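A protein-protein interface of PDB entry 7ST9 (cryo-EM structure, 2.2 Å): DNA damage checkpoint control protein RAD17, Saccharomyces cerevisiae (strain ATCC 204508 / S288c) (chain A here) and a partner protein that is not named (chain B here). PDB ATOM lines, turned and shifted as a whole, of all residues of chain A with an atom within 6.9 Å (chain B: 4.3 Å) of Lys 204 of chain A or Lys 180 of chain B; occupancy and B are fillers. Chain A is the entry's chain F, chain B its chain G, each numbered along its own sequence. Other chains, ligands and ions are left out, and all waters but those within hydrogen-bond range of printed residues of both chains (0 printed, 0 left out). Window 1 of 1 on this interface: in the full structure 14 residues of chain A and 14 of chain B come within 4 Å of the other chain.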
ATOM      1  N   SER A 165      28.386   6.109 -15.108  1.00  0.00           N
ATOM      2  CA  SER A 165      27.667   4.928 -15.577  1.00  0.00           C
ATOM      3  C   SER A 165      26.408   4.690 -14.751  1.00  0.00           C
ATOM      4  O   SER A 165      25.349   4.362 -15.300  1.00  0.00           O
ATOM      5  CB  SER A 165      28.582   3.705 -15.526  1.00  0.00           C
ATOM      6  OG  SER A 165      29.815   3.963 -16.172  1.00  0.00           O
ATOM      7  N   ALA A 166      26.507   4.844 -13.430  1.00  0.00           N
ATOM      8  CA  ALA A 166      25.335   4.665 -12.579  1.00  0.00           C
ATOM      9  C   ALA A 166      24.253   5.688 -12.909  1.00  0.00           C
ATOM     10  O   ALA A 166      23.064   5.351 -12.970  1.00  0.00           O
ATOM     11  CB  ALA A 166      25.734   4.765 -11.108  1.00  0.00           C
ATOM     12  N   ASP A 169      22.565   4.687 -16.111  1.00  0.00           N
ATOM     13  CA  ASP A 169      21.656   3.566 -15.900  1.00  0.00           C
ATOM     14  C   ASP A 169      20.364   4.028 -15.240  1.00  0.00           C
ATOM     15  O   ASP A 169      19.271   3.599 -15.628  1.00  0.00           O
ATOM     16  CB  ASP A 169      22.333   2.489 -15.055  1.00  0.00           C
ATOM     17  CG  ASP A 169      21.561   1.183 -15.047  1.00  0.00           C
ATOM     18  OD1 ASP A 169      20.631   1.045 -14.224  1.00  0.00           O
ATOM     19  OD2 ASP A 169      21.879   0.297 -15.866  1.00  0.00           O
ATOM     20  N   LEU A 170      20.469   4.903 -14.239  1.00  0.00           N
ATOM     21  CA  LEU A 170      19.269   5.426 -13.595  1.00  0.00           C
ATOM     22  C   LEU A 170      18.418   6.220 -14.579  1.00  0.00           C
ATOM     23  O   LEU A 170      17.189   6.088 -14.598  1.00  0.00           O
ATOM     24  CB  LEU A 170      19.650   6.295 -12.397  1.00  0.00           C
ATOM     25  CG  LEU A 170      20.283   5.570 -11.205  1.00  0.00           C
ATOM     26  CD1 LEU A 170      20.487   6.530 -10.045  1.00  0.00           C
ATOM     27  CD2 LEU A 170      19.434   4.385 -10.779  1.00  0.00           C
ATOM     28  N   ALA A 193      25.307   2.801  -2.118  1.00  0.00           N
ATOM     29  CA  ALA A 193      24.380   2.323  -3.132  1.00  0.00           C
ATOM     30  C   ALA A 193      23.380   3.410  -3.496  1.00  0.00           C
ATOM     31  O   ALA A 193      23.104   4.319  -2.708  1.00  0.00           O
ATOM     32  CB  ALA A 193      23.630   1.071  -2.656  1.00  0.00           C
ATOM     33  N   LEU A 194      22.846   3.302  -4.710  1.00  0.00           N
ATOM     34  CA  LEU A 194      21.755   4.144  -5.183  1.00  0.00           C
ATOM     35  C   LEU A 194      20.558   3.250  -5.471  1.00  0.00           C
ATOM     36  O   LEU A 194      20.652   2.328  -6.287  1.00  0.00           O
ATOM     37  CB  LEU A 194      22.156   4.925  -6.438  1.00  0.00           C
ATOM     38  CG  LEU A 194      23.441   5.753  -6.356  1.00  0.00           C
ATOM     39  CD1 LEU A 194      23.883   6.183  -7.746  1.00  0.00           C
ATOM     40  CD2 LEU A 194      23.246   6.964  -5.458  1.00  0.00           C
ATOM     41  N   ILE A 195      19.439   3.522  -4.807  1.00  0.00           N
ATOM     42  CA  ILE A 195      18.209   2.756  -4.971  1.00  0.00           C
ATOM     43  C   ILE A 195      17.209   3.621  -5.721  1.00  0.00           C
ATOM     44  O   ILE A 195      16.909   4.742  -5.297  1.00  0.00           O
ATOM     45  CB  ILE A 195      17.644   2.301  -3.614  1.00  0.00           C
ATOM     46  CG1 ILE A 195      18.567   1.253  -2.985  1.00  0.00           C
ATOM     47  CG2 ILE A 195      16.234   1.747  -3.778  1.00  0.00           C
ATOM     48  CD1 ILE A 195      19.421   1.791  -1.865  1.00  0.00           C
ATOM     49  N   SER A 196      16.692   3.102  -6.828  1.00  0.00           N
ATOM     50  CA  SER A 196      15.811   3.850  -7.713  1.00  0.00           C
ATOM     51  C   SER A 196      14.401   3.279  -7.658  1.00  0.00           C
ATOM     52  O   SER A 196      14.213   2.061  -7.737  1.00  0.00           O
ATOM     53  CB  SER A 196      16.327   3.818  -9.153  1.00  0.00           C
ATOM     54  OG  SER A 196      16.826   2.535  -9.486  1.00  0.00           O
ATOM     55  N   PHE A 202      11.501  -1.166  -7.765  1.00  0.00           N
ATOM     56  CA  PHE A 202      12.668  -0.771  -6.988  1.00  0.00           C
ATOM     57  C   PHE A 202      13.892  -1.514  -7.507  1.00  0.00           C
ATOM     58  O   PHE A 202      13.891  -2.747  -7.575  1.00  0.00           O
ATOM     59  CB  PHE A 202      12.461  -1.062  -5.501  1.00  0.00           C
ATOM     60  CG  PHE A 202      11.678   0.000  -4.782  1.00  0.00           C
ATOM     61  CD1 PHE A 202      10.294  -0.024  -4.779  1.00  0.00           C
ATOM     62  CD2 PHE A 202      12.326   1.023  -4.114  1.00  0.00           C
ATOM     63  CE1 PHE A 202       9.571   0.952  -4.120  1.00  0.00           C
ATOM     64  CE2 PHE A 202      11.610   2.001  -3.453  1.00  0.00           C
ATOM     65  CZ  PHE A 202      10.231   1.965  -3.456  1.00  0.00           C
ATOM     66  N   SER A 203      14.927  -0.761  -7.871  1.00  0.00           N
ATOM     67  CA  SER A 203      16.176  -1.324  -8.362  1.00  0.00           C
ATOM     68  C   SER A 203      17.332  -0.752  -7.555  1.00  0.00           C
ATOM     69  O   SER A 203      17.200   0.282  -6.897  1.00  0.00           O
ATOM     70  CB  SER A 203      16.381  -1.037  -9.857  1.00  0.00           C
ATOM     71  OG  SER A 203      15.942   0.267 -10.193  1.00  0.00           O
ATOM     72  N   LYS A 204      18.472  -1.436  -7.609  1.00  0.00           N
ATOM     73  CA  LYS A 204      19.646  -1.055  -6.838  1.00  0.00           C
ATOM     74  C   LYS A 204      20.878  -1.033  -7.732  1.00  0.00           C
ATOM     75  O   LYS A 204      21.028  -1.876  -8.619  1.00  0.00           O
ATOM     76  CB  LYS A 204      19.874  -2.026  -5.670  1.00  0.00           C
ATOM     77  CG  LYS A 204      21.015  -1.637  -4.738  1.00  0.00           C
ATOM     78  CD  LYS A 204      21.514  -2.813  -3.904  1.00  0.00           C
ATOM     79  CE  LYS A 204      20.383  -3.720  -3.443  1.00  0.00           C
ATOM     80  NZ  LYS A 204      20.846  -4.723  -2.446  1.00  0.00           N
ATOM     81  N   ILE A 205      21.755  -0.059  -7.490  1.00  0.00           N
ATOM     82  CA  ILE A 205      23.086  -0.013  -8.082  1.00  0.00           C
ATOM     83  C   ILE A 205      24.077   0.135  -6.939  1.00  0.00           C
ATOM     84  O   ILE A 205      24.067   1.153  -6.235  1.00  0.00           O
ATOM     85  CB  ILE A 205      23.241   1.140  -9.089  1.00  0.00           C
ATOM     86  CG1 ILE A 205      22.061   1.161 -10.064  1.00  0.00           C
ATOM     87  CG2 ILE A 205      24.559   1.007  -9.845  1.00  0.00           C
ATOM     88  CD1 ILE A 205      22.152   2.243 -11.120  1.00  0.00           C
ATOM     89  N   LYS A 206      24.927  -0.869  -6.753  1.00  0.00           N
ATOM     90  CA  LYS A 206      25.851  -0.930  -5.629  1.00  0.00           C
ATOM     91  C   LYS A 206      27.274  -0.713  -6.122  1.00  0.00           C
ATOM     92  O   LYS A 206      27.713  -1.366  -7.075  1.00  0.00           O
ATOM     93  CB  LYS A 206      25.740  -2.275  -4.909  1.00  0.00           C
ATOM     94  CG  LYS A 206      26.518  -2.351  -3.608  1.00  0.00           C
ATOM     95  CD  LYS A 206      27.288  -3.657  -3.498  1.00  0.00           C
ATOM     96  CE  LYS A 206      27.937  -3.808  -2.133  1.00  0.00           C
ATOM     97  NZ  LYS A 206      29.417  -3.647  -2.198  1.00  0.00           N
ATOM     98  N   ILE A 324      13.610  -0.475   0.676  1.00  0.00           N
ATOM     99  CA  ILE A 324      15.040  -0.198   0.780  1.00  0.00           C
ATOM    100  C   ILE A 324      15.695  -1.150   1.773  1.00  0.00           C
ATOM    101  O   ILE A 324      16.772  -1.699   1.513  1.00  0.00           O
ATOM    102  CB  ILE A 324      15.269   1.274   1.170  1.00  0.00           C
ATOM    103  CG1 ILE A 324      14.823   2.199   0.035  1.00  0.00           C
ATOM    104  CG2 ILE A 324      16.733   1.518   1.501  1.00  0.00           C
ATOM    105  CD1 ILE A 324      14.503   3.605   0.487  1.00  0.00           C
ATOM    106  N   LEU A 326      14.668  -4.141   2.673  1.00  0.00           N
ATOM    107  CA  LEU A 326      14.707  -5.475   2.083  1.00  0.00           C
ATOM    108  C   LEU A 326      15.812  -5.583   1.040  1.00  0.00           C
ATOM    109  O   LEU A 326      16.512  -6.598   0.967  1.00  0.00           O
ATOM    110  CB  LEU A 326      13.351  -5.815   1.467  1.00  0.00           C
ATOM    111  CG  LEU A 326      12.244  -6.144   2.471  1.00  0.00           C
ATOM    112  CD1 LEU A 326      10.881  -5.835   1.880  1.00  0.00           C
ATOM    113  CD2 LEU A 326      12.328  -7.599   2.907  1.00  0.00           C
ATOM    114  N   LEU A 327      15.982  -4.542   0.221  1.00  0.00           N
ATOM    115  CA  LEU A 327      17.034  -4.556  -0.787  1.00  0.00           C
ATOM    116  C   LEU A 327      18.414  -4.630  -0.145  1.00  0.00           C
ATOM    117  O   LEU A 327      19.283  -5.377  -0.610  1.00  0.00           O
ATOM    118  CB  LEU A 327      16.923  -3.313  -1.672  1.00  0.00           C
ATOM    119  CG  LEU A 327      16.071  -3.463  -2.933  1.00  0.00           C
ATOM    120  CD1 LEU A 327      15.647  -2.100  -3.459  1.00  0.00           C
ATOM    121  CD2 LEU A 327      16.827  -4.238  -3.999  1.00  0.00           C
ATOM    122  N   MET A 328      18.633  -3.867   0.924  1.00  0.00           N
ATOM    123  CA  MET A 328      19.932  -3.835   1.585  1.00  0.00           C
ATOM    124  C   MET A 328      20.106  -4.949   2.609  1.00  0.00           C
ATOM    125  O   MET A 328      21.187  -5.059   3.199  1.00  0.00           O
ATOM    126  CB  MET A 328      20.137  -2.478   2.266  1.00  0.00           C
ATOM    127  CG  MET A 328      20.049  -1.275   1.329  1.00  0.00           C
ATOM    128  SD  MET A 328      20.635  -1.592  -0.348  1.00  0.00           S
ATOM    129  CE  MET A 328      22.398  -1.356  -0.144  1.00  0.00           C
ATOM    130  N   GLU A 329      19.086  -5.771   2.835  1.00  0.00           N
ATOM    131  CA  GLU A 329      19.195  -6.887   3.767  1.00  0.00           C
ATOM    132  C   GLU A 329      18.359  -8.069   3.291  1.00  0.00           C
ATOM    133  O   GLU A 329      18.639  -8.659   2.247  1.00  0.00           O
ATOM    134  CB  GLU A 329      18.754  -6.461   5.170  1.00  0.00           C
ATOM    135  CG  GLU A 329      19.113  -7.454   6.266  1.00  0.00           C
ATOM    136  CD  GLU A 329      20.611  -7.604   6.455  1.00  0.00           C
ATOM    137  OE1 GLU A 329      21.251  -8.294   5.635  1.00  0.00           O
ATOM    138  OE2 GLU A 329      21.148  -7.031   7.426  1.00  0.00           O
ATOM    139  N   PRO B 142      25.212  -1.953 -21.525  1.00  0.00           N
ATOM    140  CA  PRO B 142      25.496  -0.515 -21.460  1.00  0.00           C
ATOM    141  C   PRO B 142      26.524  -0.103 -22.503  1.00  0.00           C
ATOM    142  O   PRO B 142      27.410  -0.873 -22.877  1.00  0.00           O
ATOM    143  CB  PRO B 142      26.028  -0.318 -20.035  1.00  0.00           C
ATOM    144  CG  PRO B 142      25.482  -1.463 -19.265  1.00  0.00           C
ATOM    145  CD  PRO B 142      25.436  -2.610 -20.226  1.00  0.00           C
ATOM    146  N   VAL B 170      16.693 -10.122 -11.182  1.00  0.00           N
ATOM    147  CA  VAL B 170      17.732 -10.002 -12.200  1.00  0.00           C
ATOM    148  C   VAL B 170      18.934  -9.319 -11.563  1.00  0.00           C
ATOM    149  O   VAL B 170      18.820  -8.190 -11.067  1.00  0.00           O
ATOM    150  CB  VAL B 170      17.247  -9.216 -13.427  1.00  0.00           C
ATOM    151  CG1 VAL B 170      18.224  -9.390 -14.583  1.00  0.00           C
ATOM    152  CG2 VAL B 170      15.845  -9.653 -13.825  1.00  0.00           C
ATOM    153  N   VAL B 171      20.079  -9.994 -11.584  1.00  0.00           N
ATOM    154  CA  VAL B 171      21.323  -9.478 -11.022  1.00  0.00           C
ATOM    155  C   VAL B 171      22.341  -9.380 -12.150  1.00  0.00           C
ATOM    156  O   VAL B 171      22.639 -10.382 -12.814  1.00  0.00           O
ATOM    157  CB  VAL B 171      21.847 -10.368  -9.884  1.00  0.00           C
ATOM    158  CG1 VAL B 171      23.205  -9.878  -9.400  1.00  0.00           C
ATOM    159  CG2 VAL B 171      20.849 -10.402  -8.738  1.00  0.00           C
ATOM    160  N   ILE B 172      22.876  -8.181 -12.363  1.00  0.00           N
ATOM    161  CA  ILE B 172      23.841  -7.912 -13.423  1.00  0.00           C
ATOM    162  C   ILE B 172      25.147  -7.482 -12.773  1.00  0.00           C
ATOM    163  O   ILE B 172      25.181  -6.493 -12.027  1.00  0.00           O
ATOM    164  CB  ILE B 172      23.337  -6.835 -14.397  1.00  0.00           C
ATOM    165  CG1 ILE B 172      21.905  -7.142 -14.848  1.00  0.00           C
ATOM    166  CG2 ILE B 172      24.264  -6.736 -15.603  1.00  0.00           C
ATOM    167  CD1 ILE B 172      21.282  -6.049 -15.685  1.00  0.00           C
ATOM    168  N   MET B 174      28.966  -6.075 -13.390  1.00  0.00           N
ATOM    169  CA  MET B 174      29.732  -5.311 -14.361  1.00  0.00           C
ATOM    170  C   MET B 174      31.221  -5.588 -14.190  1.00  0.00           C
ATOM    171  O   MET B 174      31.685  -5.945 -13.103  1.00  0.00           O
ATOM    172  CB  MET B 174      29.459  -3.814 -14.211  1.00  0.00           C
ATOM    173  CG  MET B 174      27.981  -3.455 -14.215  1.00  0.00           C
ATOM    174  SD  MET B 174      27.121  -3.996 -15.706  1.00  0.00           S
ATOM    175  CE  MET B 174      27.873  -2.941 -16.941  1.00  0.00           C
ATOM    176  N   VAL B 179      27.361  -3.698  -9.328  1.00  0.00           N
ATOM    177  CA  VAL B 179      26.272  -4.667  -9.313  1.00  0.00           C
ATOM    178  C   VAL B 179      24.955  -3.917  -9.457  1.00  0.00           C
ATOM    179  O   VAL B 179      24.745  -2.889  -8.800  1.00  0.00           O
ATOM    180  CB  VAL B 179      26.280  -5.512  -8.025  1.00  0.00           C
ATOM    181  CG1 VAL B 179      25.112  -6.489  -8.023  1.00  0.00           C
ATOM    182  CG2 VAL B 179      27.600  -6.251  -7.884  1.00  0.00           C
ATOM    183  N   LYS B 180      24.079  -4.425 -10.319  1.00  0.00           N
ATOM    184  CA  LYS B 180      22.746  -3.878 -10.517  1.00  0.00           C
ATOM    185  C   LYS B 180      21.711  -4.956 -10.226  1.00  0.00           C
ATOM    186  O   LYS B 180      21.895  -6.119 -10.597  1.00  0.00           O
ATOM    187  CB  LYS B 180      22.571  -3.350 -11.945  1.00  0.00           C
ATOM    188  CG  LYS B 180      23.221  -1.998 -12.185  1.00  0.00           C
ATOM    189  CD  LYS B 180      24.009  -1.973 -13.484  1.00  0.00           C
ATOM    190  CE  LYS B 180      23.115  -2.222 -14.685  1.00  0.00           C
ATOM    191  NZ  LYS B 180      23.737  -1.748 -15.950  1.00  0.00           N
ATOM    192  N   GLU B 181      20.628  -4.571  -9.555  1.00  0.00           N
ATOM    193  CA  GLU B 181      19.582  -5.503  -9.156  1.00  0.00           C
ATOM    194  C   GLU B 181      18.225  -4.956  -9.572  1.00  0.00           C
ATOM    195  O   GLU B 181      17.930  -3.778  -9.343  1.00  0.00           O
ATOM    196  CB  GLU B 181      19.613  -5.748  -7.644  1.00  0.00           C
ATOM    197  CG  GLU B 181      18.667  -6.841  -7.173  1.00  0.00           C
ATOM    198  CD  GLU B 181      19.220  -7.631  -6.000  1.00  0.00           C
ATOM    199  OE1 GLU B 181      20.094  -7.103  -5.282  1.00  0.00           O
ATOM    200  OE2 GLU B 181      18.779  -8.781  -5.796  1.00  0.00           O
ATOM    201  N   TYR B 182      17.406  -5.813 -10.180  1.00  0.00           N
ATOM    202  CA  TYR B 182      16.051  -5.464 -10.586  1.00  0.00           C
ATOM    203  C   TYR B 182      15.093  -6.563 -10.151  1.00  0.00           C
ATOM    204  O   TYR B 182      15.458  -7.740 -10.105  1.00  0.00           O
ATOM    205  CB  TYR B 182      15.945  -5.267 -12.106  1.00  0.00           C
ATOM    206  CG  TYR B 182      16.950  -4.298 -12.689  1.00  0.00           C
ATOM    207  CD1 TYR B 182      18.200  -4.732 -13.106  1.00  0.00           C
ATOM    208  CD2 TYR B 182      16.641  -2.953 -12.835  1.00  0.00           C
ATOM    209  CE1 TYR B 182      19.117  -3.852 -13.646  1.00  0.00           C
ATOM    210  CE2 TYR B 182      17.550  -2.065 -13.372  1.00  0.00           C
ATOM    211  CZ  TYR B 182      18.787  -2.520 -13.778  1.00  0.00           C
ATOM    212  OH  TYR B 182      19.696  -1.640 -14.313  1.00  0.00           O
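Of the 18 printed residues of chain A, 5 touch a printed residue of chain B. Hydrophobic or aromatic side chains of chain A that line the printed part of chain B: Ile 205. Hydrophobic or aromatic side chains of chain B that line the printed part of chain A: Tyr 182. Among the printed residues, Asp or Glu carboxylates within 4 Å of a Lys or Arg side-chain nitrogen of the other chain: Asp 169 of chain A with Lys 180 of chain B (2.8 Å) and Lys 204 of chain A with Glu 181 of chain B (3.8 Å).
The side-chain amino group (NZ) of Lys 180 of chain B lies within salt-bridge range of the side-chain carboxylate (OD2) of Asp 169 of chain A, 2.8 Å away. The side-chain carboxylate (OD1) of Asp 169 of chain A sits at hydrogen-bond distance from the side-chain hydroxyl (OH) of Tyr 182 of chain B, 2.8 Å away. The side-chain amino group (NZ) of Lys 204 of chain A lies within salt-bridge range of the side-chain carboxylate (OE1) of Glu 181 of chain B (3.8 Å). The backbone carbonyl oxygen (O) of Val 179 of chain B lies within hydrogen-bond range of the backbone NH (N) of Lys 206 of chain A, 2.9 Å away.
Printed residues of chain B within 4 Å of Ser 203 of chain A: Glu 181 (3.2 Å) and Tyr 182 (3.6 Å). Lys 204 of chain A touches just these residues of chain B: Val 179, Lys 180 and Glu 181. Of the printed residues of chain B, Ile 205 of chain A touches Val 179 and Lys 180. Printed residues of chain B within 4 Å of Lys 206 of chain A: Val 179. Met 174 of chain B touches none of the printed residues of chain A. Of the printed residues of chain A, Glu 181 of chain B touches Ser 203 (3.2 Å) and Lys 204 (2.9 Å). Printed residues of chain A within 4 Å of Tyr 182 of chain B: Asp 169 and Ser 203. The nearest residue of chain A that does not touch Lys 180 of chain B is Lys 206 of chain A (5.1 Å).
Among the printed residues, merely in contact across the chains: Ser 203 of chain A with Glu 181 of chain B, Ser 203 of chain A with Tyr 182 of chain B, Lys 204 of chain A with Val 179 of chain B, Lys 204 of chain A with Lys 180 of chain B, Ile 205 of chain A with Val 179 of chain B and Ile 205 of chain A with Lys 180 of chain B.
N of Ile 205 of chain A lies within hydrogen-bond range of O of Leu 194 of chain A, 2.9 Å away. OG of Ser 196 of chain A lies within hydrogen-bond range of OG of Ser 203 of chain A (2.5 Å). The side-chain amino group of Lys 204 of chain A lies within hydrogen-bond range of the backbone carbonyl oxygen of Leu 327 of chain A. The side-chain sulfur (SD) of Met 328 of chain A sits close to the side-chain amino group (NZ) of Lys 204 of chain A. O of Tyr 182 of chain B sits at hydrogen-bond distance from N of Val 170 of chain B (2.9 Å). The backbone NH (N) of Ile 172 of chain B is in hydrogen-bond range of the backbone carbonyl oxygen (O) of Lys 180 of chain B (2.9 Å).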
